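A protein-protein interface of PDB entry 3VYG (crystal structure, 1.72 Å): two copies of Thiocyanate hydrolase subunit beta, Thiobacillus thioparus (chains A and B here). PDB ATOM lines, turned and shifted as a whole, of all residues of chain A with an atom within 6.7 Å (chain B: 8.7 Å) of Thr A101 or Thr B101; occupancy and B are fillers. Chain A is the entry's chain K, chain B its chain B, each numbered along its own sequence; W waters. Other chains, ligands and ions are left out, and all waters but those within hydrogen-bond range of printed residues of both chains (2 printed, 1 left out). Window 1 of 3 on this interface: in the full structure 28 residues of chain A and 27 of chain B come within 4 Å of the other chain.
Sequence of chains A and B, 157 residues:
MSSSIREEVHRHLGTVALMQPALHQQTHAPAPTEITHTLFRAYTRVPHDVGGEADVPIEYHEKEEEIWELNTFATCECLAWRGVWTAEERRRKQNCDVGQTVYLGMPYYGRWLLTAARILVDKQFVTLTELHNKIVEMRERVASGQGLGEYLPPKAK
Hydrophobic or aromatic side chains of chain B that line the printed part of chain A: Pro B30, Tyr B43, Val B102, Leu B104 and Met B106.
Printed residues of chain A that touch a printed residue of chain B: Thr A27, Tyr A43, Gln A100, Thr A101, Val A102, Leu A104, Gly A105 and Met A106.
Among the printed residues, no Asp or Glu carboxylate lies within 4 Å of a Lys or Arg side-chain nitrogen of the other chain.
Among the printed residues, pairs that only touch across the chains: Gly A105 with Pro B30 (3.2 Å), Leu A104 with Pro B30 (3.4 Å), Val A102 with Tyr B43 (3.4 Å), Tyr A43 with Val B102 (3.4 Å), Tyr A43 with Gly B105 (3.6 Å), Tyr A43 with Met B106 (3.6 Å), Gly A105 with Tyr B43 (3.6 Å), Leu A104 with Thr B27 (3.6 Å), Met A106 with Tyr B43 (3.6 Å), Thr A101 with Gln B100 (3.7 Å), Gln A100 with Thr B101 (3.7 Å), Met A106 with Ala B29 (3.7 Å), Thr A27 with Gly B105 (3.8 Å), Leu A104 with His B28 (3.8 Å), Met A106 with Pro B30 (3.9 Å) and Thr A101 with Tyr B43 (3.98 Å).
The side-chain amide nitrogen of Gln B100 sits close to the guanidinium group of Arg B45 (2.8 Å).
Water W2 lies within hydrogen-bond range of the side-chain hydroxyl (OH) of Tyr A43 (2.8 Å) and the backbone carbonyl oxygen (O) of Gly B105 (2.9 Å).
Water W1 bridges O of Gly A105 (2.9 Å) and OH of Tyr B43 (2.9 Å).
Thr A27 touches Gly B105, but with the chains exchanged Gly A105 does not touch Thr B27 (4.1 Å).
Tyr A43 touches Val B102, and with the chains exchanged Val A102 touches Tyr B43.
Tyr A43 touches Gly B105, and with the chains exchanged Gly A105 touches Tyr B43.
Thr A101 touches its own counterpart, Thr B101.
Of the 19 pairs that touch across the chains among the printed residues, 11 have their exchanged pair printed and touching as well.
O of Leu A104 lies within hydrogen-bond range of N of Ala B29 (2.8 Å).
OG1 of Thr A101 lies within hydrogen-bond range of OG1 of Thr B101.
O of Thr A27 sits close to O of Leu B104 (3.3 Å).
Thr A101 touches just these residues of chain B: Tyr B43, Gln B100 and Thr B101.
Of the printed residues of chain A, Thr B101 touches Gln A100 and Thr A101.
Printed residues of chain A within 4 Å of Pro B30: Leu A104 (3.4 Å), Gly A105 (3.2 Å) and Met A106 (3.9 Å).
Of the printed residues of chain A, Val B102 touches Tyr A43.
Printed residues of chain B within 4 Å of Met A106: Ala B29, Pro B30 and Tyr B43.
The nearest residue of chain B that does not touch Thr A101 is Thr B27 (5.3 Å).
The nearest printed residue of chain B that does not touch Gln A100 is Val B98 (5.8 Å).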
ATOM      1  N   THR A  27       9.961  23.272  22.185  1.00  0.00           N
ATOM      2  CA  THR A  27       9.136  24.468  22.170  1.00  0.00           C
ATOM      3  C   THR A  27       7.960  24.229  21.228  1.00  0.00           C
ATOM      4  O   THR A  27       8.169  23.909  20.086  1.00  0.00           O
ATOM      5  CB  THR A  27       9.959  25.715  21.627  1.00  0.00           C
ATOM      6  OG1 THR A  27      10.592  25.280  20.418  1.00  0.00           O
ATOM      7  CG2 THR A  27      10.999  26.118  22.737  1.00  0.00           C
ATOM      8  N   TYR A  43      15.650  34.474  18.639  1.00  0.00           N
ATOM      9  CA  TYR A  43      14.834  33.809  17.601  1.00  0.00           C
ATOM     10  C   TYR A  43      14.862  34.605  16.320  1.00  0.00           C
ATOM     11  O   TYR A  43      14.820  34.003  15.212  1.00  0.00           O
ATOM     12  CB  TYR A  43      13.344  33.657  18.033  1.00  0.00           C
ATOM     13  CG  TYR A  43      13.186  32.408  18.844  1.00  0.00           C
ATOM     14  CD1 TYR A  43      12.708  32.493  20.175  1.00  0.00           C
ATOM     15  CD2 TYR A  43      13.498  31.153  18.321  1.00  0.00           C
ATOM     16  CE1 TYR A  43      12.568  31.377  20.956  1.00  0.00           C
ATOM     17  CE2 TYR A  43      13.310  29.984  19.127  1.00  0.00           C
ATOM     18  CZ  TYR A  43      12.801  30.133  20.415  1.00  0.00           C
ATOM     19  OH  TYR A  43      12.672  28.985  21.236  1.00  0.00           O
ATOM     20  N   PRO A  47      20.836  33.804  10.874  1.00  0.00           N
ATOM     21  CA  PRO A  47      21.695  32.740  11.349  1.00  0.00           C
ATOM     22  C   PRO A  47      23.105  32.706  10.815  1.00  0.00           C
ATOM     23  O   PRO A  47      23.933  31.963  11.300  1.00  0.00           O
ATOM     24  CB  PRO A  47      21.003  31.455  10.890  1.00  0.00           C
ATOM     25  CG  PRO A  47      19.917  31.899   9.974  1.00  0.00           C
ATOM     26  CD  PRO A  47      19.548  33.303  10.294  1.00  0.00           C
ATOM     27  N   VAL A  98      16.661  31.199   4.893  1.00  0.00           N
ATOM     28  CA  VAL A  98      16.468  29.747   4.990  1.00  0.00           C
ATOM     29  C   VAL A  98      16.120  29.344   6.446  1.00  0.00           C
ATOM     30  O   VAL A  98      15.497  28.271   6.651  1.00  0.00           O
ATOM     31  CB  VAL A  98      17.634  28.878   4.559  1.00  0.00           C
ATOM     32  CG1 VAL A  98      17.916  29.052   2.996  1.00  0.00           C
ATOM     33  CG2 VAL A  98      18.881  29.152   5.354  1.00  0.00           C
ATOM     34  N   GLY A  99      16.519  30.183   7.430  1.00  0.00           N
ATOM     35  CA  GLY A  99      16.178  29.893   8.871  1.00  0.00           C
ATOM     36  C   GLY A  99      17.234  28.962   9.494  1.00  0.00           C
ATOM     37  O   GLY A  99      17.953  28.221   8.826  1.00  0.00           O
ATOM     38  N   GLN A 100      17.278  28.979  10.832  1.00  0.00           N
ATOM     39  CA  GLN A 100      18.346  28.277  11.614  1.00  0.00           C
ATOM     40  C   GLN A 100      18.507  26.767  11.365  1.00  0.00           C
ATOM     41  O   GLN A 100      19.614  26.275  11.194  1.00  0.00           O
ATOM     42  CB  GLN A 100      18.026  28.537  13.081  1.00  0.00           C
ATOM     43  CG  GLN A 100      18.944  27.931  14.099  1.00  0.00           C
ATOM     44  CD  GLN A 100      20.385  28.504  13.978  1.00  0.00           C
ATOM     45  OE1 GLN A 100      21.176  28.107  13.120  1.00  0.00           O
ATOM     46  NE2 GLN A 100      20.688  29.407  14.855  1.00  0.00           N
ATOM     47  N   THR A 101      17.372  26.059  11.268  1.00  0.00           N
ATOM     48  CA  THR A 101      17.432  24.576  11.066  1.00  0.00           C
ATOM     49  C   THR A 101      18.102  24.190   9.725  1.00  0.00           C
ATOM     50  O   THR A 101      19.067  23.421   9.642  1.00  0.00           O
ATOM     51  CB  THR A 101      16.018  23.979  11.209  1.00  0.00           C
ATOM     52  OG1 THR A 101      15.577  24.081  12.568  1.00  0.00           O
ATOM     53  CG2 THR A 101      16.059  22.455  10.856  1.00  0.00           C
ATOM     54  N   VAL A 102      17.569  24.679   8.605  1.00  0.00           N
ATOM     55  CA  VAL A 102      18.165  24.375   7.254  1.00  0.00           C
ATOM     56  C   VAL A 102      19.566  24.970   7.149  1.00  0.00           C
ATOM     57  O   VAL A 102      20.480  24.351   6.576  1.00  0.00           O
ATOM     58  CB  VAL A 102      17.250  24.961   6.206  1.00  0.00           C
ATOM     59  CG1 VAL A 102      17.950  25.004   4.841  1.00  0.00           C
ATOM     60  CG2 VAL A 102      16.012  24.037   6.100  1.00  0.00           C
ATOM     61  N   TYR A 103      19.796  26.111   7.846  1.00  0.00           N
ATOM     62  CA  TYR A 103      21.106  26.795   7.763  1.00  0.00           C
ATOM     63  C   TYR A 103      22.272  25.853   8.196  1.00  0.00           C
ATOM     64  O   TYR A 103      23.319  25.762   7.536  1.00  0.00           O
ATOM     65  CB  TYR A 103      21.088  28.122   8.548  1.00  0.00           C
ATOM     66  CG  TYR A 103      22.408  28.837   8.374  1.00  0.00           C
ATOM     67  CD1 TYR A 103      22.757  29.370   7.107  1.00  0.00           C
ATOM     68  CD2 TYR A 103      23.322  28.867   9.414  1.00  0.00           C
ATOM     69  CE1 TYR A 103      23.992  29.990   6.913  1.00  0.00           C
ATOM     70  CE2 TYR A 103      24.587  29.443   9.216  1.00  0.00           C
ATOM     71  CZ  TYR A 103      24.892  30.035   7.955  1.00  0.00           C
ATOM     72  OH  TYR A 103      26.145  30.583   7.739  1.00  0.00           O
ATOM     73  N   LEU A 104      22.025  25.076   9.255  1.00  0.00           N
ATOM     74  CA  LEU A 104      23.042  24.134   9.728  1.00  0.00           C
ATOM     75  C   LEU A 104      22.727  22.677   9.386  1.00  0.00           C
ATOM     76  O   LEU A 104      23.630  21.841   9.424  1.00  0.00           O
ATOM     77  CB  LEU A 104      23.296  24.319  11.196  1.00  0.00           C
ATOM     78  CG  LEU A 104      23.934  25.632  11.592  1.00  0.00           C
ATOM     79  CD1 LEU A 104      23.950  25.949  13.145  1.00  0.00           C
ATOM     80  CD2 LEU A 104      25.345  25.595  11.051  1.00  0.00           C
ATOM     81  N   GLY A 105      21.482  22.349   9.086  1.00  0.00           N
ATOM     82  CA  GLY A 105      21.225  20.965   8.678  1.00  0.00           C
ATOM     83  C   GLY A 105      21.526  20.567   7.272  1.00  0.00           C
ATOM     84  O   GLY A 105      21.789  19.381   6.978  1.00  0.00           O
ATOM     85  N   MET A 106      21.518  21.502   6.290  1.00  0.00           N
ATOM     86  CA  MET A 106      21.718  21.175   4.943  1.00  0.00           C
ATOM     87  C   MET A 106      23.165  21.593   4.586  1.00  0.00           C
ATOM     88  O   MET A 106      23.822  22.297   5.451  1.00  0.00           O
ATOM     89  CB  MET A 106      20.675  21.930   4.111  1.00  0.00           C
ATOM     90  CG  MET A 106      19.257  21.235   4.314  1.00  0.00           C
ATOM     91  SD  MET A 106      19.205  19.664   3.349  1.00  0.00           S
ATOM     92  CE  MET A 106      19.093  20.433   1.781  1.00  0.00           C
ATOM     93  N   THR B  27      23.863  19.142  14.643  1.00  0.00           N
ATOM     94  CA  THR B  27      24.135  19.123  13.203  1.00  0.00           C
ATOM     95  C   THR B  27      24.942  20.346  12.729  1.00  0.00           C
ATOM     96  O   THR B  27      24.516  21.467  13.019  1.00  0.00           O
ATOM     97  CB  THR B  27      22.806  19.074  12.416  1.00  0.00           C
ATOM     98  OG1 THR B  27      22.106  20.271  12.627  1.00  0.00           O
ATOM     99  CG2 THR B  27      21.858  18.146  13.134  1.00  0.00           C
ATOM    100  N   HIS B  28      26.060  20.155  12.017  1.00  0.00           N
ATOM    101  CA  HIS B  28      26.891  21.349  11.643  1.00  0.00           C
ATOM    102  C   HIS B  28      27.324  21.437  10.133  1.00  0.00           C
ATOM    103  O   HIS B  28      28.478  21.245   9.765  1.00  0.00           O
ATOM    104  CB  HIS B  28      28.155  21.468  12.516  1.00  0.00           C
ATOM    105  CG  HIS B  28      27.885  21.831  13.943  1.00  0.00           C
ATOM    106  ND1 HIS B  28      27.873  20.912  14.977  1.00  0.00           N
ATOM    107  CD2 HIS B  28      27.638  23.036  14.506  1.00  0.00           C
ATOM    108  CE1 HIS B  28      27.612  21.539  16.120  1.00  0.00           C
ATOM    109  NE2 HIS B  28      27.480  22.827  15.862  1.00  0.00           N
ATOM    110  N   ALA B  29      26.406  21.856   9.312  1.00  0.00           N
ATOM    111  CA  ALA B  29      26.646  21.902   7.879  1.00  0.00           C
ATOM    112  C   ALA B  29      27.347  20.644   7.329  1.00  0.00           C
ATOM    113  O   ALA B  29      28.474  20.639   6.976  1.00  0.00           O
ATOM    114  CB  ALA B  29      27.387  23.200   7.527  1.00  0.00           C
ATOM    115  N   PRO B  30      26.636  19.552   7.263  1.00  0.00           N
ATOM    116  CA  PRO B  30      27.190  18.289   6.739  1.00  0.00           C
ATOM    117  C   PRO B  30      27.529  18.359   5.265  1.00  0.00           C
ATOM    118  O   PRO B  30      26.983  19.214   4.529  1.00  0.00           O
ATOM    119  CB  PRO B  30      26.036  17.278   7.031  1.00  0.00           C
ATOM    120  CG  PRO B  30      24.786  18.162   6.900  1.00  0.00           C
ATOM    121  CD  PRO B  30      25.221  19.437   7.674  1.00  0.00           C
ATOM    122  N   ALA B  42      13.052  15.696   4.710  1.00  0.00           N
ATOM    123  CA  ALA B  42      12.701  16.237   5.977  1.00  0.00           C
ATOM    124  C   ALA B  42      13.189  17.678   6.210  1.00  0.00           C
ATOM    125  O   ALA B  42      12.481  18.429   6.875  1.00  0.00           O
ATOM    126  CB  ALA B  42      13.168  15.341   7.103  1.00  0.00           C
ATOM    127  N   TYR B  43      14.352  18.033   5.674  1.00  0.00           N
ATOM    128  CA  TYR B  43      14.800  19.429   5.824  1.00  0.00           C
ATOM    129  C   TYR B  43      14.046  20.343   4.878  1.00  0.00           C
ATOM    130  O   TYR B  43      13.876  21.555   5.219  1.00  0.00           O
ATOM    131  CB  TYR B  43      16.302  19.538   5.505  1.00  0.00           C
ATOM    132  CG  TYR B  43      17.125  19.115   6.691  1.00  0.00           C
ATOM    133  CD1 TYR B  43      17.983  18.026   6.605  1.00  0.00           C
ATOM    134  CD2 TYR B  43      17.076  19.805   7.908  1.00  0.00           C
ATOM    135  CE1 TYR B  43      18.745  17.602   7.695  1.00  0.00           C
ATOM    136  CE2 TYR B  43      17.844  19.434   8.987  1.00  0.00           C
ATOM    137  CZ  TYR B  43      18.650  18.288   8.892  1.00  0.00           C
ATOM    138  OH  TYR B  43      19.414  17.903   9.971  1.00  0.00           O
ATOM    139  N   THR B  44      13.616  19.842   3.699  1.00  0.00           N
ATOM    140  CA  THR B  44      12.869  20.743   2.760  1.00  0.00           C
ATOM    141  C   THR B  44      11.335  20.724   2.921  1.00  0.00           C
ATOM    142  O   THR B  44      10.623  21.305   2.121  1.00  0.00           O
ATOM    143  CB  THR B  44      13.223  20.395   1.255  1.00  0.00           C
ATOM    144  OG1 THR B  44      12.885  19.029   0.973  1.00  0.00           O
ATOM    145  CG2 THR B  44      14.708  20.617   0.985  1.00  0.00           C
ATOM    146  N   ARG B  45      10.860  20.054   3.966  1.00  0.00           N
ATOM    147  CA  ARG B  45       9.432  19.913   4.292  1.00  0.00           C
ATOM    148  C   ARG B  45       8.931  21.352   4.525  1.00  0.00           C
ATOM    149  O   ARG B  45       9.702  22.258   4.904  1.00  0.00           O
ATOM    150  CB  ARG B  45       9.255  19.191   5.662  1.00  0.00           C
ATOM    151  CG  ARG B  45       9.684  20.179   6.819  1.00  0.00           C
ATOM    152  CD  ARG B  45       9.523  19.754   8.298  1.00  0.00           C
ATOM    153  NE  ARG B  45       8.128  19.480   8.519  1.00  0.00           N
ATOM    154  CZ  ARG B  45       7.516  19.366   9.677  1.00  0.00           C
ATOM    155  NH1 ARG B  45       8.142  19.523  10.840  1.00  0.00           N
ATOM    156  NH2 ARG B  45       6.246  19.083   9.651  1.00  0.00           N
ATOM    157  N   PRO B  47       7.055  23.581   7.045  1.00  0.00           N
ATOM    158  CA  PRO B  47       6.874  23.454   8.498  1.00  0.00           C
ATOM    159  C   PRO B  47       5.464  23.307   8.991  1.00  0.00           C
ATOM    160  O   PRO B  47       5.184  22.674  10.036  1.00  0.00           O
ATOM    161  CB  PRO B  47       7.575  24.748   9.089  1.00  0.00           C
ATOM    162  CG  PRO B  47       8.586  25.005   7.964  1.00  0.00           C
ATOM    163  CD  PRO B  47       8.014  24.644   6.707  1.00  0.00           C
ATOM    164  N   CYS B  96       5.451  28.978   6.634  1.00  0.00           N
ATOM    165  CA  CYS B  96       6.374  28.024   5.927  1.00  0.00           C
ATOM    166  C   CYS B  96       7.719  28.695   5.793  1.00  0.00           C
ATOM    167  O   CYS B  96       8.792  28.180   6.218  1.00  0.00           O
ATOM    168  CB  CYS B  96       5.871  27.613   4.556  1.00  0.00           C
ATOM    169  SG  CYS B  96       4.270  26.785   4.719  1.00  0.00           S
ATOM    170  N   ASP B  97       7.717  29.930   5.244  1.00  0.00           N
ATOM    171  CA  ASP B  97       9.042  30.439   5.009  1.00  0.00           C
ATOM    172  C   ASP B  97       9.837  30.892   6.232  1.00  0.00           C
ATOM    173  O   ASP B  97      11.094  30.978   6.146  1.00  0.00           O
ATOM    174  CB  ASP B  97       8.934  31.790   4.200  1.00  0.00           C
ATOM    175  CG  ASP B  97       8.434  31.603   2.740  1.00  0.00           C
ATOM    176  OD1 ASP B  97       8.359  30.454   2.223  1.00  0.00           O
ATOM    177  OD2 ASP B  97       8.151  32.729   2.130  1.00  0.00           O
ATOM    178  N   VAL B  98       9.177  31.080   7.366  1.00  0.00           N
ATOM    179  CA  VAL B  98       9.891  31.277   8.615  1.00  0.00           C
ATOM    180  C   VAL B  98      10.848  30.220   9.067  1.00  0.00           C
ATOM    181  O   VAL B  98      11.828  30.595   9.774  1.00  0.00           O
ATOM    182  CB  VAL B  98       8.979  31.668   9.815  1.00  0.00           C
ATOM    183  CG1 VAL B  98       8.120  33.035   9.520  1.00  0.00           C
ATOM    184  CG2 VAL B  98       8.040  30.565  10.100  1.00  0.00           C
ATOM    185  N   GLY B  99      10.693  29.017   8.556  1.00  0.00           N
ATOM    186  CA  GLY B  99      11.547  27.898   8.878  1.00  0.00           C
ATOM    187  C   GLY B  99      11.233  27.260  10.259  1.00  0.00           C
ATOM    188  O   GLY B  99      10.564  27.880  11.063  1.00  0.00           O
ATOM    189  N   GLN B 100      11.688  25.992  10.427  1.00  0.00           N
ATOM    190  CA  GLN B 100      11.240  25.188  11.588  1.00  0.00           C
ATOM    191  C   GLN B 100      11.487  25.806  12.974  1.00  0.00           C
ATOM    192  O   GLN B 100      10.642  25.707  13.838  1.00  0.00           O
ATOM    193  CB  GLN B 100      12.043  23.920  11.502  1.00  0.00           C
ATOM    194  CG  GLN B 100      11.721  22.956  12.509  1.00  0.00           C
ATOM    195  CD  GLN B 100      10.316  22.341  12.273  1.00  0.00           C
ATOM    196  OE1 GLN B 100       9.317  22.966  12.595  1.00  0.00           O
ATOM    197  NE2 GLN B 100      10.271  21.055  11.866  1.00  0.00           N
ATOM    198  N   THR B 101      12.652  26.440  13.191  1.00  0.00           N
ATOM    199  CA  THR B 101      12.997  26.984  14.500  1.00  0.00           C
ATOM    200  C   THR B 101      12.074  28.072  14.925  1.00  0.00           C
ATOM    201  O   THR B 101      11.529  28.075  16.020  1.00  0.00           O
ATOM    202  CB  THR B 101      14.493  27.431  14.544  1.00  0.00           C
ATOM    203  OG1 THR B 101      15.335  26.279  14.365  1.00  0.00           O
ATOM    204  CG2 THR B 101      14.751  28.068  15.918  1.00  0.00           C
ATOM    205  N   VAL B 102      11.932  29.135  14.114  1.00  0.00           N
ATOM    206  CA  VAL B 102      10.954  30.114  14.461  1.00  0.00           C
ATOM    207  C   VAL B 102       9.515  29.635  14.442  1.00  0.00           C
ATOM    208  O   VAL B 102       8.723  30.053  15.239  1.00  0.00           O
ATOM    209  CB  VAL B 102      11.113  31.295  13.472  1.00  0.00           C
ATOM    210  CG1 VAL B 102       9.962  32.319  13.596  1.00  0.00           C
ATOM    211  CG2 VAL B 102      12.484  31.923  13.758  1.00  0.00           C
ATOM    212  N   TYR B 103       9.174  28.741  13.508  1.00  0.00           N
ATOM    213  CA  TYR B 103       7.818  28.252  13.397  1.00  0.00           C
ATOM    214  C   TYR B 103       7.295  27.664  14.724  1.00  0.00           C
ATOM    215  O   TYR B 103       6.180  27.926  15.136  1.00  0.00           O
ATOM    216  CB  TYR B 103       7.784  27.165  12.359  1.00  0.00           C
ATOM    217  CG  TYR B 103       6.344  26.715  12.134  1.00  0.00           C
ATOM    218  CD1 TYR B 103       5.396  27.612  11.665  1.00  0.00           C
ATOM    219  CD2 TYR B 103       5.940  25.393  12.454  1.00  0.00           C
ATOM    220  CE1 TYR B 103       4.050  27.233  11.480  1.00  0.00           C
ATOM    221  CE2 TYR B 103       4.594  25.021  12.257  1.00  0.00           C
ATOM    222  CZ  TYR B 103       3.676  25.918  11.797  1.00  0.00           C
ATOM    223  OH  TYR B 103       2.335  25.564  11.685  1.00  0.00           O
ATOM    224  N   LEU B 104       8.152  26.940  15.445  1.00  0.00           N
ATOM    225  CA  LEU B 104       7.701  26.337  16.740  1.00  0.00           C
ATOM    226  C   LEU B 104       8.268  27.090  17.976  1.00  0.00           C
ATOM    227  O   LEU B 104       7.728  26.981  19.102  1.00  0.00           O
ATOM    228  CB  LEU B 104       8.160  24.833  16.725  1.00  0.00           C
ATOM    229  CG  LEU B 104       7.163  24.028  15.871  1.00  0.00           C
ATOM    230  CD1 LEU B 104       7.696  22.598  15.601  1.00  0.00           C
ATOM    231  CD2 LEU B 104       5.720  24.025  16.537  1.00  0.00           C
ATOM    232  N   GLY B 105       9.345  27.900  17.805  1.00  0.00           N
ATOM    233  CA  GLY B 105       9.887  28.663  18.955  1.00  0.00           C
ATOM    234  C   GLY B 105       9.176  29.950  19.310  1.00  0.00           C
ATOM    235  O   GLY B 105       9.156  30.291  20.454  1.00  0.00           O
ATOM    236  N   MET B 106       8.547  30.621  18.337  1.00  0.00           N
ATOM    237  CA  MET B 106       7.873  31.876  18.604  1.00  0.00           C
ATOM    238  C   MET B 106       6.390  31.713  18.722  1.00  0.00           C
ATOM    239  O   MET B 106       5.879  30.592  18.418  1.00  0.00           O
ATOM    240  CB  MET B 106       8.192  32.866  17.459  1.00  0.00           C
ATOM    241  CG  MET B 106       9.674  33.286  17.525  1.00  0.00           C
ATOM    242  SD  MET B 106       9.960  34.548  18.827  1.00  0.00           S
ATOM    243  CE  MET B 106       9.390  35.970  17.872  1.00  0.00           C
ATOM    244  N   PRO B 107       5.703  32.702  19.274  1.00  0.00           N
ATOM    245  CA  PRO B 107       4.233  32.629  19.397  1.00  0.00           C
ATOM    246  C   PRO B 107       3.498  32.798  18.074  1.00  0.00           C
ATOM    247  O   PRO B 107       4.009  33.420  17.161  1.00  0.00           O
ATOM    248  CB  PRO B 107       3.860  33.781  20.355  1.00  0.00           C
ATOM    249  CG  PRO B 107       5.221  34.259  20.925  1.00  0.00           C
ATOM    250  CD  PRO B 107       6.187  33.990  19.804  1.00  0.00           C
ATOM    251  N   ARG B 111       4.432  35.270  14.829  1.00  0.00           N
ATOM    252  CA  ARG B 111       4.700  34.956  13.395  1.00  0.00           C
ATOM    253  C   ARG B 111       3.844  35.832  12.467  1.00  0.00           C
ATOM    254  O   ARG B 111       4.339  36.311  11.410  1.00  0.00           O
ATOM    255  CB  ARG B 111       4.546  33.462  13.055  1.00  0.00           C
ATOM    256  CG  ARG B 111       5.560  32.650  13.848  1.00  0.00           C
ATOM    257  CD  ARG B 111       5.502  31.138  13.612  1.00  0.00           C
ATOM    258  NE  ARG B 111       4.172  30.605  13.957  1.00  0.00           N
ATOM    259  CZ  ARG B 111       3.173  30.396  13.105  1.00  0.00           C
ATOM    260  NH1 ARG B 111       3.298  30.732  11.798  1.00  0.00           N
ATOM    261  NH2 ARG B 111       2.051  29.849  13.557  1.00  0.00           N
HETATM  262  O   HOH W   1      22.006  17.150   8.843  1.00  0.00           O
HETATM  263  O   HOH W   2      10.420  29.467  22.892  1.00  0.00           O
